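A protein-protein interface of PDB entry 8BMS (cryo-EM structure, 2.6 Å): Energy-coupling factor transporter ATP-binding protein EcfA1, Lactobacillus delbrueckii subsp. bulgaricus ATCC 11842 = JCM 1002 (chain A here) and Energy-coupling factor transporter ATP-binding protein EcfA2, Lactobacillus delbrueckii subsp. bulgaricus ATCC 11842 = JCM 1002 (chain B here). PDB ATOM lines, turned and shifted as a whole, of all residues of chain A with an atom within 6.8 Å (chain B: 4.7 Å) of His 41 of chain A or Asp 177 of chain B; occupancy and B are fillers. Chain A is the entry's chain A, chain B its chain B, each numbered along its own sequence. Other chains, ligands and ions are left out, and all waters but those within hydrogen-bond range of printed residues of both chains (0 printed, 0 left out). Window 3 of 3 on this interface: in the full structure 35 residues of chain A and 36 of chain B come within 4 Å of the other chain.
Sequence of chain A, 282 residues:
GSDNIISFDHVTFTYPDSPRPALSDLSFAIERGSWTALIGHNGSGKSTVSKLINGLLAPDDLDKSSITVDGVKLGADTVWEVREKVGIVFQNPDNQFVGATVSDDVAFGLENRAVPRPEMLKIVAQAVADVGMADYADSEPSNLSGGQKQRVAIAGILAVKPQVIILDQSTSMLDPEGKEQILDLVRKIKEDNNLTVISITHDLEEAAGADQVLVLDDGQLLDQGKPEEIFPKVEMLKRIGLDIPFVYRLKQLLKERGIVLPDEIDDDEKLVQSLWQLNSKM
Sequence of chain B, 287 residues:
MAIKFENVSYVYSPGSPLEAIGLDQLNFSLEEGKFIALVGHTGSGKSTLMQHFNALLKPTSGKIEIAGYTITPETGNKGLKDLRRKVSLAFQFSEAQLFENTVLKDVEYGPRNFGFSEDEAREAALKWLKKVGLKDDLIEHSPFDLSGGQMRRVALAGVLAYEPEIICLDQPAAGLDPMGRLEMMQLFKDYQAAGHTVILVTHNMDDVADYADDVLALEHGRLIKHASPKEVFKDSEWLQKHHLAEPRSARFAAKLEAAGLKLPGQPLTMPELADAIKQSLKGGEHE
The side-chain amide oxygen (OD1) of Asn 42 of chain A lies within hydrogen-bond range of the guanidinium group (NH2) of Arg 153 of chain B (3.0 Å). ND2 of Asn 42 of chain A is in hydrogen-bond range of O of Gly 175 of chain B, 3.0 Å away. The side-chain amide oxygen (OD1) of Asn 42 of chain A sits close to the side-chain carboxylate (OD1) of Asp 177 of chain B, 2.8 Å away. O of Gly 241 of chain A sits at hydrogen-bond distance from N of Met 179 of chain B. The backbone carbonyl oxygen (O) of Gly 241 of chain A lies close to the side-chain carboxylate (OD2) of Asp 177 of chain B (2.8 Å).
O of Gly 40 of chain A lies close to ND1 of His 202 of chain A. O of His 41 of chain A lies within hydrogen-bond range of OG of Ser 44 of chain A. O of His 41 of chain A is in hydrogen-bond range of NZ of Lys 46 of chain A (3.1 Å). The side-chain carboxylate (OD1) of Asp 217 of chain A lies close to a ring nitrogen (NE2) of His 41 of chain A. N of Asp 218 of chain A is in hydrogen-bond range of NE2 of His 41 of chain A (3.3 Å). NE2 of His 202 of chain A sits at hydrogen-bond distance from ND2 of Asn 42 of chain A (3.1 Å).
Among the printed residues, merely in contact across the chains: His 41 of chain A with Asp 177 of chain B (3.9 Å), Asn 42 of chain A with Leu 176 of chain B (3.5 Å), His 202 of chain A with Gly 175 of chain B (3.5 Å), His 202 of chain A with Leu 176 of chain B (3.6 Å), His 202 of chain A with Asp 177 of chain B (3.5 Å), His 202 of chain A with Pro 178 of chain B (3.7 Å) and Gly 241 of chain A with Pro 178 of chain B (3.97 Å).
His 41 of chain A touches one residue of chain B. Printed residues of chain A within 4 Å of Arg 153 of chain B: Asn 42. Of the printed residues of chain A, Gly 175 of chain B touches Asn 42 (3.0 Å) and His 202 (3.5 Å). Of chain A, only His 41, Asn 42, His 202 and Gly 241 come within 4 Å of Asp 177 of chain B. Of the printed residues of chain A, Pro 178 of chain B touches His 202 (3.7 Å) and Gly 241 (3.97 Å). The nearest residue of chain A that does not touch Asp 177 of chain B is Gly 40 of chain A (4.3 Å). The nearest printed residue of chain A that does not touch Leu 176 of chain B is Gly 40 of chain A (6.8 Å).
Among the printed residues, 12 pairs touch across the chains.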
ATOM      1  N   ILE A  39      20.116 -23.272 -21.477  1.00  0.00           N
ATOM      2  CA  ILE A  39      19.053 -23.846 -20.666  1.00  0.00           C
ATOM      3  C   ILE A  39      18.968 -23.083 -19.353  1.00  0.00           C
ATOM      4  O   ILE A  39      19.918 -22.427 -18.918  1.00  0.00           O
ATOM      5  CB  ILE A  39      19.262 -25.354 -20.409  1.00  0.00           C
ATOM      6  CG1 ILE A  39      20.461 -25.582 -19.488  1.00  0.00           C
ATOM      7  CG2 ILE A  39      19.445 -26.103 -21.717  1.00  0.00           C
ATOM      8  CD1 ILE A  39      20.661 -27.026 -19.100  1.00  0.00           C
ATOM      9  N   GLY A  40      17.803 -23.175 -18.727  1.00  0.00           N
ATOM     10  CA  GLY A  40      17.551 -22.483 -17.479  1.00  0.00           C
ATOM     11  C   GLY A  40      16.070 -22.481 -17.188  1.00  0.00           C
ATOM     12  O   GLY A  40      15.240 -22.783 -18.049  1.00  0.00           O
ATOM     13  N   HIS A  41      15.747 -22.131 -15.948  1.00  0.00           N
ATOM     14  CA  HIS A  41      14.357 -22.106 -15.525  1.00  0.00           C
ATOM     15  C   HIS A  41      13.605 -20.978 -16.231  1.00  0.00           C
ATOM     16  O   HIS A  41      14.184 -20.147 -16.936  1.00  0.00           O
ATOM     17  CB  HIS A  41      14.258 -21.939 -14.009  1.00  0.00           C
ATOM     18  CG  HIS A  41      14.795 -20.636 -13.507  1.00  0.00           C
ATOM     19  ND1 HIS A  41      14.012 -19.509 -13.377  1.00  0.00           N
ATOM     20  CD2 HIS A  41      16.036 -20.279 -13.097  1.00  0.00           C
ATOM     21  CE1 HIS A  41      14.746 -18.514 -12.913  1.00  0.00           C
ATOM     22  NE2 HIS A  41      15.979 -18.956 -12.735  1.00  0.00           N
ATOM     23  N   ASN A  42      12.290 -20.963 -16.043  1.00  0.00           N
ATOM     24  CA  ASN A  42      11.479 -19.874 -16.569  1.00  0.00           C
ATOM     25  C   ASN A  42      11.778 -18.593 -15.802  1.00  0.00           C
ATOM     26  O   ASN A  42      11.735 -18.571 -14.569  1.00  0.00           O
ATOM     27  CB  ASN A  42       9.993 -20.218 -16.467  1.00  0.00           C
ATOM     28  CG  ASN A  42       9.601 -21.386 -17.347  1.00  0.00           C
ATOM     29  OD1 ASN A  42       8.744 -22.188 -16.983  1.00  0.00           O
ATOM     30  ND2 ASN A  42      10.222 -21.486 -18.511  1.00  0.00           N
ATOM     31  N   GLY A  43      12.078 -17.523 -16.534  1.00  0.00           N
ATOM     32  CA  GLY A  43      12.405 -16.250 -15.935  1.00  0.00           C
ATOM     33  C   GLY A  43      13.877 -15.898 -15.933  1.00  0.00           C
ATOM     34  O   GLY A  43      14.215 -14.737 -15.679  1.00  0.00           O
ATOM     35  N   SER A  44      14.762 -16.857 -16.186  1.00  0.00           N
ATOM     36  CA  SER A  44      16.157 -16.537 -16.447  1.00  0.00           C
ATOM     37  C   SER A  44      16.276 -15.987 -17.861  1.00  0.00           C
ATOM     38  O   SER A  44      15.658 -16.502 -18.792  1.00  0.00           O
ATOM     39  CB  SER A  44      17.039 -17.773 -16.275  1.00  0.00           C
ATOM     40  OG  SER A  44      16.551 -18.861 -17.036  1.00  0.00           O
ATOM     41  N   GLY A  45      17.077 -14.942 -18.026  1.00  0.00           N
ATOM     42  CA  GLY A  45      17.011 -14.177 -19.256  1.00  0.00           C
ATOM     43  C   GLY A  45      17.579 -14.863 -20.482  1.00  0.00           C
ATOM     44  O   GLY A  45      18.599 -14.429 -21.018  1.00  0.00           O
ATOM     45  N   LYS A  46      16.923 -15.929 -20.944  1.00  0.00           N
ATOM     46  CA  LYS A  46      17.367 -16.611 -22.157  1.00  0.00           C
ATOM     47  C   LYS A  46      16.895 -15.876 -23.408  1.00  0.00           C
ATOM     48  O   LYS A  46      17.690 -15.601 -24.316  1.00  0.00           O
ATOM     49  CB  LYS A  46      16.867 -18.056 -22.160  1.00  0.00           C
ATOM     50  CG  LYS A  46      17.364 -18.888 -20.988  1.00  0.00           C
ATOM     51  CD  LYS A  46      17.031 -20.362 -21.157  1.00  0.00           C
ATOM     52  CE  LYS A  46      15.536 -20.601 -21.277  1.00  0.00           C
ATOM     53  NZ  LYS A  46      14.820 -20.371 -19.995  1.00  0.00           N
ATOM     54  N   HIS A 202      14.050 -26.117 -23.450  1.00  0.00           N
ATOM     55  CA  HIS A 202      13.704 -26.767 -22.196  1.00  0.00           C
ATOM     56  C   HIS A 202      13.735 -28.282 -22.309  1.00  0.00           C
ATOM     57  O   HIS A 202      13.457 -28.972 -21.322  1.00  0.00           O
ATOM     58  CB  HIS A 202      12.319 -26.310 -21.722  1.00  0.00           C
ATOM     59  CG  HIS A 202      12.294 -24.910 -21.192  1.00  0.00           C
ATOM     60  ND1 HIS A 202      13.020 -24.518 -20.090  1.00  0.00           N
ATOM     61  CD2 HIS A 202      11.628 -23.809 -21.614  1.00  0.00           C
ATOM     62  CE1 HIS A 202      12.803 -23.237 -19.854  1.00  0.00           C
ATOM     63  NE2 HIS A 202      11.962 -22.784 -20.765  1.00  0.00           N
ATOM     64  N   LEU A 216      21.702 -21.104 -17.059  1.00  0.00           N
ATOM     65  CA  LEU A 216      21.363 -19.745 -16.668  1.00  0.00           C
ATOM     66  C   LEU A 216      20.411 -19.793 -15.481  1.00  0.00           C
ATOM     67  O   LEU A 216      19.448 -20.568 -15.481  1.00  0.00           O
ATOM     68  CB  LEU A 216      20.736 -18.996 -17.846  1.00  0.00           C
ATOM     69  CG  LEU A 216      20.651 -17.473 -17.796  1.00  0.00           C
ATOM     70  CD1 LEU A 216      22.043 -16.879 -17.739  1.00  0.00           C
ATOM     71  CD2 LEU A 216      19.913 -16.965 -19.014  1.00  0.00           C
ATOM     72  N   ASP A 217      20.690 -18.975 -14.469  1.00  0.00           N
ATOM     73  CA  ASP A 217      19.917 -18.954 -13.233  1.00  0.00           C
ATOM     74  C   ASP A 217      19.809 -17.514 -12.763  1.00  0.00           C
ATOM     75  O   ASP A 217      20.827 -16.878 -12.476  1.00  0.00           O
ATOM     76  CB  ASP A 217      20.574 -19.826 -12.160  1.00  0.00           C
ATOM     77  CG  ASP A 217      19.706 -19.993 -10.930  1.00  0.00           C
ATOM     78  OD1 ASP A 217      18.521 -20.352 -11.080  1.00  0.00           O
ATOM     79  OD2 ASP A 217      20.211 -19.765  -9.810  1.00  0.00           O
ATOM     80  N   ASP A 218      18.578 -17.002 -12.699  1.00  0.00           N
ATOM     81  CA  ASP A 218      18.311 -15.631 -12.262  1.00  0.00           C
ATOM     82  C   ASP A 218      19.122 -14.621 -13.069  1.00  0.00           C
ATOM     83  O   ASP A 218      19.604 -13.615 -12.545  1.00  0.00           O
ATOM     84  CB  ASP A 218      18.575 -15.469 -10.763  1.00  0.00           C
ATOM     85  CG  ASP A 218      17.570 -16.217  -9.910  1.00  0.00           C
ATOM     86  OD1 ASP A 218      16.416 -16.385 -10.357  1.00  0.00           O
ATOM     87  OD2 ASP A 218      17.933 -16.639  -8.792  1.00  0.00           O
ATOM     88  N   GLY A 219      19.273 -14.891 -14.363  1.00  0.00           N
ATOM     89  CA  GLY A 219      20.030 -14.002 -15.218  1.00  0.00           C
ATOM     90  C   GLY A 219      21.525 -14.037 -15.013  1.00  0.00           C
ATOM     91  O   GLY A 219      22.207 -13.067 -15.351  1.00  0.00           O
ATOM     92  N   ILE A 240      17.789 -25.570  -9.289  1.00  0.00           N
ATOM     93  CA  ILE A 240      17.503 -24.367 -10.063  1.00  0.00           C
ATOM     94  C   ILE A 240      16.312 -24.552 -10.997  1.00  0.00           C
ATOM     95  O   ILE A 240      16.046 -23.684 -11.833  1.00  0.00           O
ATOM     96  CB  ILE A 240      18.742 -23.914 -10.849  1.00  0.00           C
ATOM     97  CG1 ILE A 240      19.166 -25.002 -11.832  1.00  0.00           C
ATOM     98  CG2 ILE A 240      19.879 -23.583  -9.900  1.00  0.00           C
ATOM     99  CD1 ILE A 240      20.267 -24.580 -12.756  1.00  0.00           C
ATOM    100  N   GLY A 241      15.587 -25.660 -10.878  1.00  0.00           N
ATOM    101  CA  GLY A 241      14.416 -25.884 -11.696  1.00  0.00           C
ATOM    102  C   GLY A 241      14.643 -26.689 -12.954  1.00  0.00           C
ATOM    103  O   GLY A 241      13.737 -26.764 -13.791  1.00  0.00           O
ATOM    104  N   LEU A 242      15.818 -27.280 -13.122  1.00  0.00           N
ATOM    105  CA  LEU A 242      16.118 -28.122 -14.266  1.00  0.00           C
ATOM    106  C   LEU A 242      16.059 -29.591 -13.851  1.00  0.00           C
ATOM    107  O   LEU A 242      15.652 -29.932 -12.736  1.00  0.00           O
ATOM    108  CB  LEU A 242      17.479 -27.744 -14.853  1.00  0.00           C
ATOM    109  CG  LEU A 242      17.597 -26.331 -15.425  1.00  0.00           C
ATOM    110  CD1 LEU A 242      19.002 -26.075 -15.935  1.00  0.00           C
ATOM    111  CD2 LEU A 242      16.577 -26.115 -16.529  1.00  0.00           C
ATOM    112  N   ARG B 153       2.193 -20.325 -16.918  1.00  0.00           N
ATOM    113  CA  ARG B 153       1.782 -20.574 -15.540  1.00  0.00           C
ATOM    114  C   ARG B 153       0.604 -19.694 -15.143  1.00  0.00           C
ATOM    115  O   ARG B 153      -0.316 -20.151 -14.453  1.00  0.00           O
ATOM    116  CB  ARG B 153       2.965 -20.356 -14.597  1.00  0.00           C
ATOM    117  CG  ARG B 153       4.013 -21.448 -14.679  1.00  0.00           C
ATOM    118  CD  ARG B 153       5.291 -21.067 -13.957  1.00  0.00           C
ATOM    119  NE  ARG B 153       6.431 -21.827 -14.455  1.00  0.00           N
ATOM    120  CZ  ARG B 153       6.957 -22.878 -13.843  1.00  0.00           C
ATOM    121  NH1 ARG B 153       6.474 -23.322 -12.695  1.00  0.00           N
ATOM    122  NH2 ARG B 153       7.991 -23.502 -14.398  1.00  0.00           N
ATOM    123  N   GLY B 175       6.889 -24.688 -23.149  1.00  0.00           N
ATOM    124  CA  GLY B 175       7.473 -23.500 -22.573  1.00  0.00           C
ATOM    125  C   GLY B 175       7.831 -23.606 -21.107  1.00  0.00           C
ATOM    126  O   GLY B 175       8.439 -22.674 -20.566  1.00  0.00           O
ATOM    127  N   LEU B 176       7.482 -24.707 -20.449  1.00  0.00           N
ATOM    128  CA  LEU B 176       7.763 -24.886 -19.033  1.00  0.00           C
ATOM    129  C   LEU B 176       9.079 -25.626 -18.839  1.00  0.00           C
ATOM    130  O   LEU B 176       9.391 -26.568 -19.573  1.00  0.00           O
ATOM    131  CB  LEU B 176       6.633 -25.657 -18.353  1.00  0.00           C
ATOM    132  CG  LEU B 176       5.255 -24.997 -18.356  1.00  0.00           C
ATOM    133  CD1 LEU B 176       4.235 -25.940 -17.768  1.00  0.00           C
ATOM    134  CD2 LEU B 176       5.279 -23.689 -17.588  1.00  0.00           C
ATOM    135  N   ASP B 177       9.845 -25.194 -17.841  1.00  0.00           N
ATOM    136  CA  ASP B 177      11.101 -25.846 -17.521  1.00  0.00           C
ATOM    137  C   ASP B 177      10.836 -27.239 -16.952  1.00  0.00           C
ATOM    138  O   ASP B 177       9.727 -27.530 -16.498  1.00  0.00           O
ATOM    139  CB  ASP B 177      11.903 -24.993 -16.538  1.00  0.00           C
ATOM    140  CG  ASP B 177      11.124 -24.657 -15.285  1.00  0.00           C
ATOM    141  OD1 ASP B 177       9.986 -24.163 -15.406  1.00  0.00           O
ATOM    142  OD2 ASP B 177      11.654 -24.876 -14.178  1.00  0.00           O
ATOM    143  N   PRO B 178      11.836 -28.130 -17.000  1.00  0.00           N
ATOM    144  CA  PRO B 178      11.611 -29.519 -16.551  1.00  0.00           C
ATOM    145  C   PRO B 178      10.932 -29.659 -15.195  1.00  0.00           C
ATOM    146  O   PRO B 178       9.956 -30.414 -15.070  1.00  0.00           O
ATOM    147  CB  PRO B 178      13.030 -30.092 -16.536  1.00  0.00           C
ATOM    148  CG  PRO B 178      13.736 -29.352 -17.608  1.00  0.00           C
ATOM    149  CD  PRO B 178      13.146 -27.971 -17.657  1.00  0.00           C
ATOM    150  N   MET B 179      11.425 -28.960 -14.170  1.00  0.00           N
ATOM    151  CA  MET B 179      10.792 -29.040 -12.858  1.00  0.00           C
ATOM    152  C   MET B 179       9.365 -28.510 -12.906  1.00  0.00           C
ATOM    153  O   MET B 179       8.447 -29.127 -12.353  1.00  0.00           O
ATOM    154  CB  MET B 179      11.616 -28.271 -11.827  1.00  0.00           C
ATOM    155  CG  MET B 179      10.857 -27.925 -10.557  1.00  0.00           C
ATOM    156  SD  MET B 179      11.363 -26.352  -9.834  1.00  0.00           S
ATOM    157  CE  MET B 179      10.370 -25.207 -10.788  1.00  0.00           C
ATOM    158  N   GLY B 180       9.159 -27.376 -13.576  1.00  0.00           N
ATOM    159  CA  GLY B 180       7.812 -26.854 -13.728  1.00  0.00           C
ATOM    160  C   GLY B 180       6.916 -27.782 -14.523  1.00  0.00           C
ATOM    161  O   GLY B 180       5.733 -27.931 -14.215  1.00  0.00           O
ATOM    162  N   ARG B 181       7.471 -28.424 -15.551  1.00  0.00           N
ATOM    163  CA  ARG B 181       6.703 -29.377 -16.347  1.00  0.00           C
ATOM    164  C   ARG B 181       6.221 -30.544 -15.493  1.00  0.00           C
ATOM    165  O   ARG B 181       5.039 -30.912 -15.527  1.00  0.00           O
ATOM    166  CB  ARG B 181       7.562 -29.875 -17.508  1.00  0.00           C
ATOM    167  CG  ARG B 181       6.789 -30.475 -18.658  1.00  0.00           C
ATOM    168  CD  ARG B 181       7.727 -30.870 -19.791  1.00  0.00           C
ATOM    169  NE  ARG B 181       7.028 -31.226 -21.023  1.00  0.00           N
ATOM    170  CZ  ARG B 181       6.143 -32.206 -21.145  1.00  0.00           C
ATOM    171  NH1 ARG B 181       5.851 -33.011 -20.136  1.00  0.00           N
ATOM    172  NH2 ARG B 181       5.542 -32.394 -22.317  1.00  0.00           N
